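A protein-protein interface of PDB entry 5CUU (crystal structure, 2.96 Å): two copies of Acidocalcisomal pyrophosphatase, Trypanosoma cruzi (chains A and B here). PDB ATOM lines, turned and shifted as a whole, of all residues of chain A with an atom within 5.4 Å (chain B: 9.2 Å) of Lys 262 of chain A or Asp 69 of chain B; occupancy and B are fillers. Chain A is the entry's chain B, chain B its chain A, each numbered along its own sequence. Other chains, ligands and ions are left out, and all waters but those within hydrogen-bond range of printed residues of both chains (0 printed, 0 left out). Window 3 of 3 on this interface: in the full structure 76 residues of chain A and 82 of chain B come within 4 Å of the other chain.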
ATOM      1  N   ARG A 235       2.077  15.393  18.615  1.00  0.00           N
ATOM      2  CA  ARG A 235       2.112  14.865  17.251  1.00  0.00           C
ATOM      3  C   ARG A 235       3.154  15.498  16.338  1.00  0.00           C
ATOM      4  O   ARG A 235       3.259  15.092  15.194  1.00  0.00           O
ATOM      5  CB  ARG A 235       0.720  14.924  16.600  1.00  0.00           C
ATOM      6  CG  ARG A 235       0.256  16.289  16.249  1.00  0.00           C
ATOM      7  CD  ARG A 235      -1.123  16.241  15.664  1.00  0.00           C
ATOM      8  NE  ARG A 235      -2.085  15.728  16.623  1.00  0.00           N
ATOM      9  CZ  ARG A 235      -3.282  15.258  16.301  1.00  0.00           C
ATOM     10  NH1 ARG A 235      -3.670  15.225  15.041  1.00  0.00           N
ATOM     11  NH2 ARG A 235      -4.095  14.829  17.236  1.00  0.00           N
ATOM     12  N   PHE A 260       3.881  17.201  11.205  1.00  0.00           N
ATOM     13  CA  PHE A 260       3.173  16.598  12.328  1.00  0.00           C
ATOM     14  C   PHE A 260       2.464  15.330  11.855  1.00  0.00           C
ATOM     15  O   PHE A 260       1.974  15.284  10.732  1.00  0.00           O
ATOM     16  CB  PHE A 260       2.098  17.554  12.867  1.00  0.00           C
ATOM     17  CG  PHE A 260       2.618  18.900  13.305  1.00  0.00           C
ATOM     18  CD1 PHE A 260       3.165  19.787  12.401  1.00  0.00           C
ATOM     19  CD2 PHE A 260       2.538  19.290  14.621  1.00  0.00           C
ATOM     20  CE1 PHE A 260       3.620  21.023  12.791  1.00  0.00           C
ATOM     21  CE2 PHE A 260       2.999  20.554  15.027  1.00  0.00           C
ATOM     22  CZ  PHE A 260       3.541  21.415  14.100  1.00  0.00           C
ATOM     23  N   TYR A 261       2.423  14.303  12.705  1.00  0.00           N
ATOM     24  CA  TYR A 261       1.710  13.062  12.398  1.00  0.00           C
ATOM     25  C   TYR A 261       0.236  13.459  12.249  1.00  0.00           C
ATOM     26  O   TYR A 261      -0.308  14.090  13.131  1.00  0.00           O
ATOM     27  CB  TYR A 261       1.873  12.070  13.548  1.00  0.00           C
ATOM     28  CG  TYR A 261       3.219  11.379  13.587  1.00  0.00           C
ATOM     29  CD1 TYR A 261       3.580  10.428  12.616  1.00  0.00           C
ATOM     30  CD2 TYR A 261       4.132  11.645  14.614  1.00  0.00           C
ATOM     31  CE1 TYR A 261       4.825   9.755  12.673  1.00  0.00           C
ATOM     32  CE2 TYR A 261       5.399  10.967  14.692  1.00  0.00           C
ATOM     33  CZ  TYR A 261       5.731  10.029  13.724  1.00  0.00           C
ATOM     34  OH  TYR A 261       6.931   9.353  13.817  1.00  0.00           O
ATOM     35  N   LYS A 262      -0.421  13.112  11.144  1.00  0.00           N
ATOM     36  CA  LYS A 262      -1.831  13.520  10.962  1.00  0.00           C
ATOM     37  C   LYS A 262      -2.872  12.527  11.491  1.00  0.00           C
ATOM     38  O   LYS A 262      -4.025  12.857  11.712  1.00  0.00           O
ATOM     39  CB  LYS A 262      -2.104  13.843   9.481  1.00  0.00           C
ATOM     40  CG  LYS A 262      -1.424  15.127   8.948  1.00  0.00           C
ATOM     41  CD  LYS A 262      -1.930  16.374   9.680  1.00  0.00           C
ATOM     42  CE  LYS A 262      -1.541  17.723   8.994  1.00  0.00           C
ATOM     43  NZ  LYS A 262      -0.225  18.366   9.409  1.00  0.00           N
ATOM     44  N   HIS A 263      -2.434  11.303  11.699  1.00  0.00           N
ATOM     45  CA  HIS A 263      -3.290  10.254  12.214  1.00  0.00           C
ATOM     46  C   HIS A 263      -3.699  10.544  13.654  1.00  0.00           C
ATOM     47  O   HIS A 263      -4.746  10.126  14.106  1.00  0.00           O
ATOM     48  CB  HIS A 263      -2.535   8.928  12.120  1.00  0.00           C
ATOM     49  CG  HIS A 263      -3.141   7.820  12.923  1.00  0.00           C
ATOM     50  ND1 HIS A 263      -4.429   7.369  12.719  1.00  0.00           N
ATOM     51  CD2 HIS A 263      -2.620   7.045  13.908  1.00  0.00           C
ATOM     52  CE1 HIS A 263      -4.673   6.364  13.547  1.00  0.00           C
ATOM     53  NE2 HIS A 263      -3.592   6.149  14.279  1.00  0.00           N
ATOM     54  N   GLY A 264      -2.866  11.273  14.370  1.00  0.00           N
ATOM     55  CA  GLY A 264      -3.153  11.574  15.755  1.00  0.00           C
ATOM     56  C   GLY A 264      -1.853  11.807  16.493  1.00  0.00           C
ATOM     57  O   GLY A 264      -0.796  11.885  15.860  1.00  0.00           O
ATOM     58  N   CYS A 371      -4.294   7.987   6.751  1.00  0.00           N
ATOM     59  CA  CYS A 371      -4.947   9.299   6.764  1.00  0.00           C
ATOM     60  C   CYS A 371      -4.331  10.183   5.718  1.00  0.00           C
ATOM     61  O   CYS A 371      -4.832  11.242   5.374  1.00  0.00           O
ATOM     62  CB  CYS A 371      -4.792   9.975   8.126  1.00  0.00           C
ATOM     63  SG  CYS A 371      -5.610  11.621   8.250  1.00  0.00           S
ATOM     64  N   GLN A 372      -3.212   9.743   5.211  1.00  0.00           N
ATOM     65  CA  GLN A 372      -2.538  10.527   4.216  1.00  0.00           C
ATOM     66  C   GLN A 372      -2.785   9.910   2.819  1.00  0.00           C
ATOM     67  O   GLN A 372      -2.432  10.491   1.778  1.00  0.00           O
ATOM     68  CB  GLN A 372      -1.055  10.578   4.597  1.00  0.00           C
ATOM     69  CG  GLN A 372      -0.846  10.904   6.081  1.00  0.00           C
ATOM     70  CD  GLN A 372       0.564  11.398   6.406  1.00  0.00           C
ATOM     71  OE1 GLN A 372       0.741  12.378   7.163  1.00  0.00           O
ATOM     72  NE2 GLN A 372       1.578  10.717   5.848  1.00  0.00           N
ATOM     73  N   GLU B  52      -5.841  30.786   3.450  1.00  0.00           N
ATOM     74  CA  GLU B  52      -6.544  29.544   3.780  1.00  0.00           C
ATOM     75  C   GLU B  52      -6.827  29.391   5.281  1.00  0.00           C
ATOM     76  O   GLU B  52      -7.538  28.472   5.699  1.00  0.00           O
ATOM     77  CB  GLU B  52      -5.736  28.353   3.257  1.00  0.00           C
ATOM     78  CG  GLU B  52      -4.261  28.688   2.966  1.00  0.00           C
ATOM     79  CD  GLU B  52      -3.973  29.112   1.517  1.00  0.00           C
ATOM     80  OE1 GLU B  52      -4.150  28.277   0.591  1.00  0.00           O
ATOM     81  OE2 GLU B  52      -3.548  30.271   1.312  1.00  0.00           O
ATOM     82  N   LYS B  55      -9.758  32.539   6.015  1.00  0.00           N
ATOM     83  CA  LYS B  55     -10.985  31.956   5.494  1.00  0.00           C
ATOM     84  C   LYS B  55     -11.659  31.153   6.606  1.00  0.00           C
ATOM     85  O   LYS B  55     -12.818  31.424   6.963  1.00  0.00           O
ATOM     86  CB  LYS B  55     -10.653  31.040   4.294  1.00  0.00           C
ATOM     87  CG  LYS B  55     -11.724  29.958   3.894  1.00  0.00           C
ATOM     88  CD  LYS B  55     -11.115  28.514   3.764  1.00  0.00           C
ATOM     89  CE  LYS B  55     -10.008  28.407   2.683  1.00  0.00           C
ATOM     90  NZ  LYS B  55      -9.119  27.207   2.796  1.00  0.00           N
ATOM     91  N   ARG B  56     -10.904  30.196   7.164  1.00  0.00           N
ATOM     92  CA  ARG B  56     -11.372  29.295   8.220  1.00  0.00           C
ATOM     93  C   ARG B  56     -11.369  29.813   9.659  1.00  0.00           C
ATOM     94  O   ARG B  56     -11.894  29.151  10.549  1.00  0.00           O
ATOM     95  CB  ARG B  56     -10.589  27.985   8.157  1.00  0.00           C
ATOM     96  CG  ARG B  56     -10.824  27.195   6.867  1.00  0.00           C
ATOM     97  CD  ARG B  56     -10.400  25.732   7.021  1.00  0.00           C
ATOM     98  NE  ARG B  56     -10.961  25.175   8.257  1.00  0.00           N
ATOM     99  CZ  ARG B  56     -10.521  24.083   8.881  1.00  0.00           C
ATOM    100  NH1 ARG B  56      -9.491  23.387   8.388  1.00  0.00           N
ATOM    101  NH2 ARG B  56     -11.099  23.721  10.027  1.00  0.00           N
ATOM    102  N   GLU B  60      -2.630  29.808  11.640  1.00  0.00           N
ATOM    103  CA  GLU B  60      -1.898  29.026  10.651  1.00  0.00           C
ATOM    104  C   GLU B  60      -1.279  27.811  11.330  1.00  0.00           C
ATOM    105  O   GLU B  60      -1.161  26.733  10.727  1.00  0.00           O
ATOM    106  CB  GLU B  60      -0.780  29.830  10.029  1.00  0.00           C
ATOM    107  CG  GLU B  60      -1.178  31.147   9.451  1.00  0.00           C
ATOM    108  CD  GLU B  60       0.032  31.880   8.937  1.00  0.00           C
ATOM    109  OE1 GLU B  60      -0.032  33.119   8.882  1.00  0.00           O
ATOM    110  OE2 GLU B  60       1.040  31.221   8.597  1.00  0.00           O
ATOM    111  N   PHE B  61      -0.864  28.004  12.579  1.00  0.00           N
ATOM    112  CA  PHE B  61      -0.288  26.939  13.377  1.00  0.00           C
ATOM    113  C   PHE B  61      -1.306  25.831  13.564  1.00  0.00           C
ATOM    114  O   PHE B  61      -1.007  24.662  13.365  1.00  0.00           O
ATOM    115  CB  PHE B  61       0.102  27.440  14.760  1.00  0.00           C
ATOM    116  CG  PHE B  61       0.754  26.387  15.613  1.00  0.00           C
ATOM    117  CD1 PHE B  61       2.013  25.878  15.272  1.00  0.00           C
ATOM    118  CD2 PHE B  61       0.094  25.853  16.716  1.00  0.00           C
ATOM    119  CE1 PHE B  61       2.594  24.859  16.005  1.00  0.00           C
ATOM    120  CE2 PHE B  61       0.660  24.831  17.461  1.00  0.00           C
ATOM    121  CZ  PHE B  61       1.911  24.332  17.104  1.00  0.00           C
ATOM    122  N   ASP B  62      -2.511  26.204  13.972  1.00  0.00           N
ATOM    123  CA  ASP B  62      -3.566  25.226  14.198  1.00  0.00           C
ATOM    124  C   ASP B  62      -3.838  24.426  12.944  1.00  0.00           C
ATOM    125  O   ASP B  62      -3.978  23.201  12.969  1.00  0.00           O
ATOM    126  CB  ASP B  62      -4.869  25.917  14.579  1.00  0.00           C
ATOM    127  CG  ASP B  62      -4.958  26.310  16.050  1.00  0.00           C
ATOM    128  OD1 ASP B  62      -4.055  26.002  16.882  1.00  0.00           O
ATOM    129  OD2 ASP B  62      -6.001  26.943  16.347  1.00  0.00           O
ATOM    130  N   LEU B  63      -3.944  25.170  11.845  1.00  0.00           N
ATOM    131  CA  LEU B  63      -4.239  24.621  10.533  1.00  0.00           C
ATOM    132  C   LEU B  63      -3.214  23.599  10.090  1.00  0.00           C
ATOM    133  O   LEU B  63      -3.562  22.476   9.749  1.00  0.00           O
ATOM    134  CB  LEU B  63      -4.330  25.758   9.500  1.00  0.00           C
ATOM    135  CG  LEU B  63      -4.648  25.244   8.085  1.00  0.00           C
ATOM    136  CD1 LEU B  63      -6.064  24.673   8.030  1.00  0.00           C
ATOM    137  CD2 LEU B  63      -4.462  26.382   7.083  1.00  0.00           C
ATOM    138  N   VAL B  64      -1.950  24.015  10.104  1.00  0.00           N
ATOM    139  CA  VAL B  64      -0.812  23.190   9.690  1.00  0.00           C
ATOM    140  C   VAL B  64      -0.647  21.835  10.447  1.00  0.00           C
ATOM    141  O   VAL B  64      -0.449  20.773   9.836  1.00  0.00           O
ATOM    142  CB  VAL B  64       0.490  24.059   9.803  1.00  0.00           C
ATOM    143  CG1 VAL B  64       0.793  24.365  11.262  1.00  0.00           C
ATOM    144  CG2 VAL B  64       1.660  23.366   9.139  1.00  0.00           C
ATOM    145  N   ALA B  65      -0.769  21.903  11.774  1.00  0.00           N
ATOM    146  CA  ALA B  65      -0.617  20.785  12.695  1.00  0.00           C
ATOM    147  C   ALA B  65      -1.864  19.938  12.925  1.00  0.00           C
ATOM    148  O   ALA B  65      -1.804  18.703  12.975  1.00  0.00           O
ATOM    149  CB  ALA B  65      -0.130  21.326  14.019  1.00  0.00           C
ATOM    150  N   TYR B  66      -3.002  20.591  13.081  1.00  0.00           N
ATOM    151  CA  TYR B  66      -4.212  19.845  13.338  1.00  0.00           C
ATOM    152  C   TYR B  66      -5.175  19.705  12.171  1.00  0.00           C
ATOM    153  O   TYR B  66      -6.154  18.988  12.286  1.00  0.00           O
ATOM    154  CB  TYR B  66      -4.912  20.452  14.528  1.00  0.00           C
ATOM    155  CG  TYR B  66      -3.986  20.604  15.712  1.00  0.00           C
ATOM    156  CD1 TYR B  66      -3.339  19.497  16.275  1.00  0.00           C
ATOM    157  CD2 TYR B  66      -3.780  21.861  16.292  1.00  0.00           C
ATOM    158  CE1 TYR B  66      -2.526  19.647  17.384  1.00  0.00           C
ATOM    159  CE2 TYR B  66      -2.975  22.019  17.392  1.00  0.00           C
ATOM    160  CZ  TYR B  66      -2.355  20.916  17.938  1.00  0.00           C
ATOM    161  OH  TYR B  66      -1.589  21.101  19.062  1.00  0.00           O
ATOM    162  N   GLY B  67      -4.910  20.396  11.061  1.00  0.00           N
ATOM    163  CA  GLY B  67      -5.754  20.285   9.884  1.00  0.00           C
ATOM    164  C   GLY B  67      -5.300  19.031   9.174  1.00  0.00           C
ATOM    165  O   GLY B  67      -4.105  18.818   8.992  1.00  0.00           O
ATOM    166  N   LYS B  68      -6.251  18.208   8.760  1.00  0.00           N
ATOM    167  CA  LYS B  68      -5.944  16.939   8.113  1.00  0.00           C
ATOM    168  C   LYS B  68      -5.379  17.058   6.736  1.00  0.00           C
ATOM    169  O   LYS B  68      -5.098  16.053   6.105  1.00  0.00           O
ATOM    170  CB  LYS B  68      -7.191  16.066   8.031  1.00  0.00           C
ATOM    171  CG  LYS B  68      -7.639  15.459   9.354  1.00  0.00           C
ATOM    172  CD  LYS B  68      -6.784  14.266   9.736  1.00  0.00           C
ATOM    173  CE  LYS B  68      -7.262  13.686  11.041  1.00  0.00           C
ATOM    174  NZ  LYS B  68      -6.199  13.776  12.068  1.00  0.00           N
ATOM    175  N   ASP B  69      -5.208  18.277   6.253  1.00  0.00           N
ATOM    176  CA  ASP B  69      -4.691  18.447   4.907  1.00  0.00           C
ATOM    177  C   ASP B  69      -3.226  18.717   4.722  1.00  0.00           C
ATOM    178  O   ASP B  69      -2.510  19.145   5.634  1.00  0.00           O
ATOM    179  CB  ASP B  69      -5.447  19.546   4.182  1.00  0.00           C
ATOM    180  CG  ASP B  69      -6.717  19.048   3.569  1.00  0.00           C
ATOM    181  OD1 ASP B  69      -6.721  17.853   3.179  1.00  0.00           O
ATOM    182  OD2 ASP B  69      -7.688  19.847   3.472  1.00  0.00           O
ATOM    183  N   GLU B  70      -2.792  18.460   3.498  1.00  0.00           N
ATOM    184  CA  GLU B  70      -1.430  18.706   3.117  1.00  0.00           C
ATOM    185  C   GLU B  70      -1.311  20.117   2.543  1.00  0.00           C
ATOM    186  O   GLU B  70      -1.975  20.464   1.567  1.00  0.00           O
ATOM    187  CB  GLU B  70      -0.968  17.668   2.093  1.00  0.00           C
ATOM    188  CG  GLU B  70      -0.378  16.442   2.745  1.00  0.00           C
ATOM    189  CD  GLU B  70       0.662  16.811   3.816  1.00  0.00           C
ATOM    190  OE1 GLU B  70       1.834  17.144   3.470  1.00  0.00           O
ATOM    191  OE2 GLU B  70       0.287  16.783   5.017  1.00  0.00           O
ATOM    192  N   PHE B  71      -0.483  20.929   3.197  1.00  0.00           N
ATOM    193  CA  PHE B  71      -0.202  22.292   2.774  1.00  0.00           C
ATOM    194  C   PHE B  71       0.089  22.247   1.289  1.00  0.00           C
ATOM    195  O   PHE B  71       1.156  21.774   0.874  1.00  0.00           O
ATOM    196  CB  PHE B  71       1.031  22.831   3.501  1.00  0.00           C
ATOM    197  CG  PHE B  71       0.727  23.962   4.424  1.00  0.00           C
ATOM    198  CD1 PHE B  71      -0.273  23.836   5.388  1.00  0.00           C
ATOM    199  CD2 PHE B  71       1.421  25.156   4.329  1.00  0.00           C
ATOM    200  CE1 PHE B  71      -0.577  24.877   6.241  1.00  0.00           C
ATOM    201  CE2 PHE B  71       1.121  26.210   5.179  1.00  0.00           C
ATOM    202  CZ  PHE B  71       0.120  26.068   6.138  1.00  0.00           C
ATOM    203  N   THR B  72      -0.870  22.728   0.501  1.00  0.00           N
ATOM    204  CA  THR B  72      -0.751  22.749  -0.951  1.00  0.00           C
ATOM    205  C   THR B  72       0.476  23.547  -1.394  1.00  0.00           C
ATOM    206  O   THR B  72       0.882  24.507  -0.731  1.00  0.00           O
ATOM    207  CB  THR B  72      -2.018  23.364  -1.594  1.00  0.00           C
ATOM    208  OG1 THR B  72      -2.087  24.765  -1.298  1.00  0.00           O
ATOM    209  CG2 THR B  72      -3.253  22.704  -1.035  1.00  0.00           C
ATOM    210  N   MET B  75       0.467  26.996  -0.686  1.00  0.00           N
ATOM    211  CA  MET B  75       0.550  27.419   0.710  1.00  0.00           C
ATOM    212  C   MET B  75       2.014  27.405   1.204  1.00  0.00           C
ATOM    213  O   MET B  75       2.402  28.235   2.027  1.00  0.00           O
ATOM    214  CB  MET B  75      -0.303  26.500   1.575  1.00  0.00           C
ATOM    215  CG  MET B  75      -1.795  26.587   1.323  1.00  0.00           C
ATOM    216  SD  MET B  75      -2.707  25.361   2.322  1.00  0.00           S
ATOM    217  CE  MET B  75      -2.685  26.114   3.999  1.00  0.00           C
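Of the 17 printed residues of chain B, 6 touch a printed residue of chain A.
Hydrophobic or aromatic side chains of chain B that line the printed part of chain A: Ala 65 and Tyr 66.
Of the 8 printed residues of chain A, 4 touch a printed residue of chain B.
Among the printed residues, no Asp or Glu carboxylate lies within 4 Å of a Lys or Arg side-chain nitrogen of the other chain.
O of Arg 235 of chain A is in hydrogen-bond range of N of Tyr 261 of chain A (2.7 Å).
Among the printed residues, pairs that only touch across the chains: Arg 235 of chain A with Ala 65 of chain B, Arg 235 of chain A with Tyr 66 of chain B, Phe 260 of chain A with Ala 65 of chain B, Lys 262 of chain A with Ala 65 of chain B, Lys 262 of chain A with Gly 67 of chain B, Lys 262 of chain A with Asp 69 of chain B and Cys 371 of chain A with Lys 68 of chain B.
No position is printed for both chains.
O of Lys 262 of chain A lies close to NZ of Lys 68 of chain B (2.4 Å).
The backbone carbonyl oxygen (O) of Val 64 of chain B is in hydrogen-bond range of the side-chain amino group (NZ) of Lys 262 of chain A, 2.5 Å away.
Of chain B, only Val 64, Ala 65, Gly 67, Lys 68 and Asp 69 come within 4 Å of Lys 262 of chain A.
Printed residues of chain B within 4 Å of Cys 371 of chain A: Lys 68.
Of the printed residues of chain A, Lys 68 of chain B touches Lys 262 and Cys 371.
Printed residues of chain A within 4 Å of Asp 69 of chain B: Lys 262 (3.8 Å).
The nearest printed residue of chain A that does not touch Asp 69 of chain B is Cys 371 of chain A (7.0 Å).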
